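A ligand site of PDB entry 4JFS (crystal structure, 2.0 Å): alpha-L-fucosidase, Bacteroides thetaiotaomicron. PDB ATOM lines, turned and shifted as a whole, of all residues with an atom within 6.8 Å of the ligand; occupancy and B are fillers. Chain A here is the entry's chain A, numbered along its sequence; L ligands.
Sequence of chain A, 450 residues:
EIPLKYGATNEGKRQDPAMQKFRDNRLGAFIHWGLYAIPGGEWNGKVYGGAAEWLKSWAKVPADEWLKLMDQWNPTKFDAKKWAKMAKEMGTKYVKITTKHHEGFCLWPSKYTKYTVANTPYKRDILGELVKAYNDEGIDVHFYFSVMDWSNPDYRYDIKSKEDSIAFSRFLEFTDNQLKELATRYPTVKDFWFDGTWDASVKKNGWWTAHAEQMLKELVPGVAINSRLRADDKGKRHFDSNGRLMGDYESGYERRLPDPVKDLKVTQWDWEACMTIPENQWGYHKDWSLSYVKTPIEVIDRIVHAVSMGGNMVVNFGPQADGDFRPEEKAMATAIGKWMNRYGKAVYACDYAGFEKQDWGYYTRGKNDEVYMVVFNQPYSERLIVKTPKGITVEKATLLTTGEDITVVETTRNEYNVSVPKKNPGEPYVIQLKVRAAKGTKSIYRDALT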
ATOM      1  N   PHE A  30      -1.959  18.055   8.732  1.00  0.00           N
ATOM      2  CA  PHE A  30      -1.192  18.745   9.752  1.00  0.00           C
ATOM      3  C   PHE A  30      -0.039  19.386   9.018  1.00  0.00           C
ATOM      4  O   PHE A  30       0.546  18.760   8.093  1.00  0.00           O
ATOM      5  CB  PHE A  30      -0.627  17.744  10.752  1.00  0.00           C
ATOM      6  CG  PHE A  30      -0.763  18.166  12.204  1.00  0.00           C
ATOM      7  CD1 PHE A  30      -0.219  19.347  12.650  1.00  0.00           C
ATOM      8  CD2 PHE A  30      -1.426  17.386  13.101  1.00  0.00           C
ATOM      9  CE1 PHE A  30      -0.392  19.758  13.965  1.00  0.00           C
ATOM     10  CE2 PHE A  30      -1.573  17.788  14.449  1.00  0.00           C
ATOM     11  CZ  PHE A  30      -1.046  18.988  14.867  1.00  0.00           C
ATOM     12  N   HIS A  32       3.639  20.930  10.025  1.00  0.00           N
ATOM     13  CA  HIS A  32       4.759  21.245  10.976  1.00  0.00           C
ATOM     14  C   HIS A  32       5.813  21.998  10.206  1.00  0.00           C
ATOM     15  O   HIS A  32       6.502  21.441   9.323  1.00  0.00           O
ATOM     16  CB  HIS A  32       5.371  19.957  11.512  1.00  0.00           C
ATOM     17  CG  HIS A  32       4.688  19.430  12.736  1.00  0.00           C
ATOM     18  ND1 HIS A  32       3.473  18.752  12.707  1.00  0.00           N
ATOM     19  CD2 HIS A  32       5.045  19.493  14.046  1.00  0.00           C
ATOM     20  CE1 HIS A  32       3.126  18.419  13.940  1.00  0.00           C
ATOM     21  NE2 HIS A  32       4.062  18.853  14.767  1.00  0.00           N
ATOM     22  N   ALA A  51      13.293  12.807  15.528  1.00  0.00           N
ATOM     23  CA  ALA A  51      12.368  13.693  14.839  1.00  0.00           C
ATOM     24  C   ALA A  51      13.043  15.058  14.624  1.00  0.00           C
ATOM     25  O   ALA A  51      13.638  15.647  15.542  1.00  0.00           O
ATOM     26  CB  ALA A  51      11.103  13.842  15.690  1.00  0.00           C
ATOM     27  N   GLU A  53      12.047  18.014  14.217  1.00  0.00           N
ATOM     28  CA  GLU A  53      11.590  19.187  14.917  1.00  0.00           C
ATOM     29  C   GLU A  53      12.138  19.281  16.337  1.00  0.00           C
ATOM     30  O   GLU A  53      12.135  20.382  16.942  1.00  0.00           O
ATOM     31  CB  GLU A  53      10.047  19.296  14.859  1.00  0.00           C
ATOM     32  CG  GLU A  53       9.304  18.327  15.735  1.00  0.00           C
ATOM     33  CD  GLU A  53       9.227  16.924  15.197  1.00  0.00           C
ATOM     34  OE1 GLU A  53       9.625  16.633  13.994  1.00  0.00           O
ATOM     35  OE2 GLU A  53       8.604  16.147  15.937  1.00  0.00           O
ATOM     36  N   TRP A  54      12.696  18.183  16.822  1.00  0.00           N
ATOM     37  CA  TRP A  54      13.397  18.086  18.105  1.00  0.00           C
ATOM     38  C   TRP A  54      14.951  18.160  17.973  1.00  0.00           C
ATOM     39  O   TRP A  54      15.680  17.931  18.932  1.00  0.00           O
ATOM     40  CB  TRP A  54      13.031  16.758  18.779  1.00  0.00           C
ATOM     41  CG  TRP A  54      11.792  16.780  19.564  1.00  0.00           C
ATOM     42  CD1 TRP A  54      10.513  16.758  19.095  1.00  0.00           C
ATOM     43  CD2 TRP A  54      11.697  16.853  20.967  1.00  0.00           C
ATOM     44  NE1 TRP A  54       9.623  16.839  20.164  1.00  0.00           N
ATOM     45  CE2 TRP A  54      10.332  16.871  21.313  1.00  0.00           C
ATOM     46  CE3 TRP A  54      12.639  16.901  21.984  1.00  0.00           C
ATOM     47  CZ2 TRP A  54       9.895  17.001  22.607  1.00  0.00           C
ATOM     48  CZ3 TRP A  54      12.199  16.972  23.284  1.00  0.00           C
ATOM     49  CH2 TRP A  54      10.856  17.014  23.581  1.00  0.00           C
ATOM     50  N   THR A  98       1.168  24.342  12.926  1.00  0.00           N
ATOM     51  CA  THR A  98       2.045  24.696  14.057  1.00  0.00           C
ATOM     52  C   THR A  98       2.224  26.222  14.130  1.00  0.00           C
ATOM     53  O   THR A  98       3.031  26.762  13.431  1.00  0.00           O
ATOM     54  CB  THR A  98       3.440  24.048  13.975  1.00  0.00           C
ATOM     55  OG1 THR A  98       4.022  24.335  12.708  1.00  0.00           O
ATOM     56  CG2 THR A  98       3.372  22.564  14.090  1.00  0.00           C
ATOM     57  N   HIS A 101       6.143  25.840  17.711  1.00  0.00           N
ATOM     58  CA  HIS A 101       6.519  24.531  18.214  1.00  0.00           C
ATOM     59  C   HIS A 101       7.437  24.782  19.462  1.00  0.00           C
ATOM     60  O   HIS A 101       7.507  25.911  19.966  1.00  0.00           O
ATOM     61  CB  HIS A 101       7.219  23.666  17.155  1.00  0.00           C
ATOM     62  CG  HIS A 101       7.093  22.186  17.401  1.00  0.00           C
ATOM     63  ND1 HIS A 101       8.016  21.453  18.106  1.00  0.00           N
ATOM     64  CD2 HIS A 101       6.117  21.316  17.048  1.00  0.00           C
ATOM     65  CE1 HIS A 101       7.613  20.202  18.182  1.00  0.00           C
ATOM     66  NE2 HIS A 101       6.470  20.095  17.511  1.00  0.00           N
ATOM     67  N   HIS A 102       8.033  23.707  19.996  1.00  0.00           N
ATOM     68  CA  HIS A 102       8.813  23.805  21.250  1.00  0.00           C
ATOM     69  C   HIS A 102       9.897  24.850  21.161  1.00  0.00           C
ATOM     70  O   HIS A 102      10.174  25.519  22.124  1.00  0.00           O
ATOM     71  CB  HIS A 102       9.439  22.456  21.667  1.00  0.00           C
ATOM     72  CG  HIS A 102       8.499  21.281  21.628  1.00  0.00           C
ATOM     73  ND1 HIS A 102       7.157  21.366  21.958  1.00  0.00           N
ATOM     74  CD2 HIS A 102       8.710  19.977  21.338  1.00  0.00           C
ATOM     75  CE1 HIS A 102       6.601  20.177  21.852  1.00  0.00           C
ATOM     76  NE2 HIS A 102       7.521  19.314  21.476  1.00  0.00           N
ATOM     77  N   TYR A 144      -2.221  24.454  16.188  1.00  0.00           N
ATOM     78  CA  TYR A 144      -1.307  23.741  17.109  1.00  0.00           C
ATOM     79  C   TYR A 144      -0.532  24.801  17.887  1.00  0.00           C
ATOM     80  O   TYR A 144      -0.172  25.820  17.348  1.00  0.00           O
ATOM     81  CB  TYR A 144      -0.307  22.843  16.285  1.00  0.00           C
ATOM     82  CG  TYR A 144       0.903  22.345  17.082  1.00  0.00           C
ATOM     83  CD1 TYR A 144       1.866  23.238  17.571  1.00  0.00           C
ATOM     84  CD2 TYR A 144       1.086  21.001  17.324  1.00  0.00           C
ATOM     85  CE1 TYR A 144       2.983  22.785  18.258  1.00  0.00           C
ATOM     86  CE2 TYR A 144       2.209  20.532  18.054  1.00  0.00           C
ATOM     87  CZ  TYR A 144       3.119  21.416  18.531  1.00  0.00           C
ATOM     88  OH  TYR A 144       4.170  20.993  19.290  1.00  0.00           O
ATOM     89  N   MET A 148       5.119  24.378  26.297  1.00  0.00           N
ATOM     90  CA  MET A 148       6.579  24.291  26.452  1.00  0.00           C
ATOM     91  C   MET A 148       7.266  25.123  25.367  1.00  0.00           C
ATOM     92  O   MET A 148       6.928  24.969  24.169  1.00  0.00           O
ATOM     93  CB  MET A 148       7.081  22.834  26.394  1.00  0.00           C
ATOM     94  CG  MET A 148       8.584  22.692  26.626  1.00  0.00           C
ATOM     95  SD  MET A 148       9.222  20.986  26.661  1.00  0.00           S
ATOM     96  CE  MET A 148       9.034  20.466  24.960  1.00  0.00           C
ATOM     97  N   TRP A 193      -5.038  23.061  19.450  1.00  0.00           N
ATOM     98  CA  TRP A 193      -4.468  21.771  19.719  1.00  0.00           C
ATOM     99  C   TRP A 193      -3.165  21.987  20.456  1.00  0.00           C
ATOM    100  O   TRP A 193      -2.164  22.348  19.871  1.00  0.00           O
ATOM    101  CB  TRP A 193      -4.277  20.996  18.389  1.00  0.00           C
ATOM    102  CG  TRP A 193      -4.050  19.503  18.558  1.00  0.00           C
ATOM    103  CD1 TRP A 193      -5.004  18.536  18.483  1.00  0.00           C
ATOM    104  CD2 TRP A 193      -2.823  18.826  18.843  1.00  0.00           C
ATOM    105  NE1 TRP A 193      -4.456  17.325  18.713  1.00  0.00           N
ATOM    106  CE2 TRP A 193      -3.120  17.450  18.913  1.00  0.00           C
ATOM    107  CE3 TRP A 193      -1.507  19.232  19.030  1.00  0.00           C
ATOM    108  CZ2 TRP A 193      -2.125  16.450  19.169  1.00  0.00           C
ATOM    109  CZ3 TRP A 193      -0.513  18.261  19.269  1.00  0.00           C
ATOM    110  CH2 TRP A 193      -0.846  16.886  19.338  1.00  0.00           C
ATOM    111  N   ASP A 195       0.230  21.138  22.731  1.00  0.00           N
ATOM    112  CA  ASP A 195       1.273  20.189  22.903  1.00  0.00           C
ATOM    113  C   ASP A 195       2.159  20.770  23.999  1.00  0.00           C
ATOM    114  O   ASP A 195       2.022  21.920  24.412  1.00  0.00           O
ATOM    115  CB  ASP A 195       2.042  20.098  21.559  1.00  0.00           C
ATOM    116  CG  ASP A 195       2.892  18.850  21.443  1.00  0.00           C
ATOM    117  OD1 ASP A 195       2.923  18.041  22.390  1.00  0.00           O
ATOM    118  OD2 ASP A 195       3.539  18.670  20.370  1.00  0.00           O
ATOM    119  N   GLY A 196       3.125  19.990  24.442  1.00  0.00           N
ATOM    120  CA  GLY A 196       4.117  20.509  25.361  1.00  0.00           C
ATOM    121  C   GLY A 196       3.470  20.893  26.682  1.00  0.00           C
ATOM    122  O   GLY A 196       3.849  21.896  27.291  1.00  0.00           O
ATOM    123  N   TRP A 198       3.074  18.263  29.130  1.00  0.00           N
ATOM    124  CA  TRP A 198       3.281  17.070  29.930  1.00  0.00           C
ATOM    125  C   TRP A 198       4.150  17.353  31.176  1.00  0.00           C
ATOM    126  O   TRP A 198       4.198  16.537  32.049  1.00  0.00           O
ATOM    127  CB  TRP A 198       3.904  15.926  29.087  1.00  0.00           C
ATOM    128  CG  TRP A 198       5.157  16.290  28.561  1.00  0.00           C
ATOM    129  CD1 TRP A 198       6.323  16.388  29.251  1.00  0.00           C
ATOM    130  CD2 TRP A 198       5.448  16.695  27.216  1.00  0.00           C
ATOM    131  NE1 TRP A 198       7.325  16.786  28.425  1.00  0.00           N
ATOM    132  CE2 TRP A 198       6.814  17.006  27.166  1.00  0.00           C
ATOM    133  CE3 TRP A 198       4.693  16.804  26.041  1.00  0.00           C
ATOM    134  CZ2 TRP A 198       7.455  17.401  26.003  1.00  0.00           C
ATOM    135  CZ3 TRP A 198       5.313  17.229  24.872  1.00  0.00           C
ATOM    136  CH2 TRP A 198       6.699  17.524  24.863  1.00  0.00           C
ATOM    137  N   ARG A 228      -5.331  17.052  25.228  1.00  0.00           N
ATOM    138  CA  ARG A 228      -3.931  17.060  25.614  1.00  0.00           C
ATOM    139  C   ARG A 228      -3.538  18.295  26.453  1.00  0.00           C
ATOM    140  O   ARG A 228      -2.599  18.253  27.256  1.00  0.00           O
ATOM    141  CB  ARG A 228      -3.120  16.995  24.348  1.00  0.00           C
ATOM    142  CG  ARG A 228      -1.706  16.566  24.575  1.00  0.00           C
ATOM    143  CD  ARG A 228      -1.003  16.328  23.240  1.00  0.00           C
ATOM    144  NE  ARG A 228      -1.501  15.191  22.424  1.00  0.00           N
ATOM    145  CZ  ARG A 228      -0.718  14.290  21.778  1.00  0.00           C
ATOM    146  NH1 ARG A 228       0.629  14.316  21.899  1.00  0.00           N
ATOM    147  NH2 ARG A 228      -1.272  13.323  21.036  1.00  0.00           N
ATOM    148  N   GLU A 254      -1.504   8.862  18.324  1.00  0.00           N
ATOM    149  CA  GLU A 254      -0.549   9.562  17.588  1.00  0.00           C
ATOM    150  C   GLU A 254       0.347   8.517  17.080  1.00  0.00           C
ATOM    151  O   GLU A 254       0.959   7.844  17.837  1.00  0.00           O
ATOM    152  CB  GLU A 254       0.146  10.512  18.546  1.00  0.00           C
ATOM    153  CG  GLU A 254       1.316  11.257  17.973  1.00  0.00           C
ATOM    154  CD  GLU A 254       2.019  11.979  19.079  1.00  0.00           C
ATOM    155  OE1 GLU A 254       1.284  12.513  19.906  1.00  0.00           O
ATOM    156  OE2 GLU A 254       3.261  11.985  19.139  1.00  0.00           O
ATOM    157  N   ARG A 255       0.349   8.288  15.792  1.00  0.00           N
ATOM    158  CA  ARG A 255       1.119   7.208  15.271  1.00  0.00           C
ATOM    159  C   ARG A 255       0.584   5.779  15.635  1.00  0.00           C
ATOM    160  O   ARG A 255       1.157   4.781  15.247  1.00  0.00           O
ATOM    161  CB  ARG A 255       2.624   7.495  15.574  1.00  0.00           C
ATOM    162  CG  ARG A 255       3.071   8.914  15.060  1.00  0.00           C
ATOM    163  CD  ARG A 255       4.561   9.178  14.994  1.00  0.00           C
ATOM    164  NE  ARG A 255       5.092   8.945  16.344  1.00  0.00           N
ATOM    165  CZ  ARG A 255       5.658   7.823  16.801  1.00  0.00           C
ATOM    166  NH1 ARG A 255       5.865   6.794  16.000  1.00  0.00           N
ATOM    167  NH2 ARG A 255       6.052   7.751  18.081  1.00  0.00           N
ATOM    168  N   CYS A 274      -3.675  11.727  14.893  1.00  0.00           N
ATOM    169  CA  CYS A 274      -2.743  12.340  13.953  1.00  0.00           C
ATOM    170  C   CYS A 274      -1.677  11.341  13.601  1.00  0.00           C
ATOM    171  O   CYS A 274      -1.404  10.402  14.355  1.00  0.00           O
ATOM    172  CB  CYS A 274      -2.124  13.590  14.532  1.00  0.00           C
ATOM    173  SG  CYS A 274      -1.258  13.399  16.084  1.00  0.00           S
ATOM    174  N   ASN A 280       8.423   8.446  12.355  1.00  0.00           N
ATOM    175  CA  ASN A 280       8.447   9.447  13.402  1.00  0.00           C
ATOM    176  C   ASN A 280       9.226  10.720  13.012  1.00  0.00           C
ATOM    177  O   ASN A 280      10.254  11.003  13.564  1.00  0.00           O
ATOM    178  CB  ASN A 280       9.053   8.819  14.659  1.00  0.00           C
ATOM    179  CG  ASN A 280       8.767   9.661  15.898  1.00  0.00           C
ATOM    180  OD1 ASN A 280       8.095  10.705  15.860  1.00  0.00           O
ATOM    181  ND2 ASN A 280       9.326   9.214  17.011  1.00  0.00           N
ATOM    182  N   TRP A 282       7.929  14.687  12.058  1.00  0.00           N
ATOM    183  CA  TRP A 282       6.871  15.665  11.871  1.00  0.00           C
ATOM    184  C   TRP A 282       7.362  16.866  11.081  1.00  0.00           C
ATOM    185  O   TRP A 282       6.775  17.232  10.059  1.00  0.00           O
ATOM    186  CB  TRP A 282       6.279  16.098  13.201  1.00  0.00           C
ATOM    187  CG  TRP A 282       5.705  14.990  13.969  1.00  0.00           C
ATOM    188  CD1 TRP A 282       6.390  14.149  14.800  1.00  0.00           C
ATOM    189  CD2 TRP A 282       4.325  14.612  14.055  1.00  0.00           C
ATOM    190  NE1 TRP A 282       5.530  13.303  15.425  1.00  0.00           N
ATOM    191  CE2 TRP A 282       4.262  13.523  14.969  1.00  0.00           C
ATOM    192  CE3 TRP A 282       3.146  15.034  13.439  1.00  0.00           C
ATOM    193  CZ2 TRP A 282       3.053  12.887  15.288  1.00  0.00           C
ATOM    194  CZ3 TRP A 282       1.934  14.387  13.745  1.00  0.00           C
ATOM    195  CH2 TRP A 282       1.900  13.326  14.652  1.00  0.00           C
ATOM    196  N   GLY A 283       8.416  17.504  11.570  1.00  0.00           N
ATOM    197  CA  GLY A 283       9.061  18.535  10.777  1.00  0.00           C
ATOM    198  C   GLY A 283       9.854  17.908   9.618  1.00  0.00           C
ATOM    199  O   GLY A 283      10.078  16.715   9.561  1.00  0.00           O
HETATM  200  C1  LIG L   1       7.392  11.249  23.255  1.00  0.00           C
HETATM  201  O1  LIG L   1       7.435  12.728  23.397  1.00  0.00           O
HETATM  202  C2  LIG L   1       6.989  13.520  22.373  1.00  0.00           C
HETATM  203  C3  LIG L   1       6.797  14.874  22.671  1.00  0.00           C
HETATM  204  C4  LIG L   1       6.329  15.752  21.694  1.00  0.00           C
HETATM  205  C5  LIG L   1       6.738  13.041  21.082  1.00  0.00           C
HETATM  206  C6  LIG L   1       6.278  13.929  20.110  1.00  0.00           C
HETATM  207  C7  LIG L   1       6.071  15.293  20.395  1.00  0.00           C
HETATM  208  C8  LIG L   1       5.571  16.233  19.425  1.00  0.00           C
HETATM  209  C9  LIG L   1       6.118  16.086  18.013  1.00  0.00           C
HETATM  210  O2  LIG L   1       7.266  16.932  17.860  1.00  0.00           O
HETATM  211  C10 LIG L   1       4.856  16.504  17.188  1.00  0.00           C
HETATM  212  O3  LIG L   1       4.622  17.975  17.216  1.00  0.00           O
HETATM  213  C11 LIG L   1       3.803  15.714  17.890  1.00  0.00           C
HETATM  214  C12 LIG L   1       2.427  16.042  17.342  1.00  0.00           C
HETATM  215  N1  LIG L   1       4.089  16.156  19.237  1.00  0.00           N
HETATM  216  C13 LIG L   1       3.296  15.433  20.244  1.00  0.00           C
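Residues that only touch the ligand: His 102 (3.8 Å), Tyr 144 (3.6 Å), Trp 193 (3.9 Å), Trp 198 (3.4 Å), Arg 228 (3.3 Å), Glu 254 (3.6 Å) and Trp 282 (3.7 Å). Hydrophobic or aromatic side chains within 4 Å of the ligand: His 32, Trp 54, His 101, Tyr 144, Trp 193, Trp 198 and Trp 282. The nearest printed residue that does not touch the ligand is Cys 274 (4.7 Å).
NE2 of His 101 sits close to OH of Tyr 144, 3.0 Å away. OE1 of Glu 53 is in hydrogen-bond range of N of Gly 283 (2.8 Å). OD2 of Asp 195 lies within hydrogen-bond range of OH of Tyr 144, 2.6 Å away. The side-chain carboxylate of Glu 254 lies within salt-bridge range of the guanidinium group of Arg 228 (2.8 Å). OE1 of Glu 53 lies within hydrogen-bond range of N of Trp 282, 3.2 Å away.
An oxygen (O2) of the ligand lies within hydrogen-bond range of the side-chain carboxylate (OE2) of Glu 53 (2.5 Å). The side-chain carboxylate (OD2) of Asp 195 is in salt-bridge range of a nitrogen (N1) of the ligand, at 2.8 Å. A ring nitrogen (NE2) of His 32 is in hydrogen-bond range of an oxygen (O3) of the ligand (2.7 Å). NE1 of Trp 54 is in hydrogen-bond range of O2 of the ligand, 3.3 Å away. A ring nitrogen (NE2) of His 101 is in hydrogen-bond range of an oxygen (O3) of the ligand (2.8 Å).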
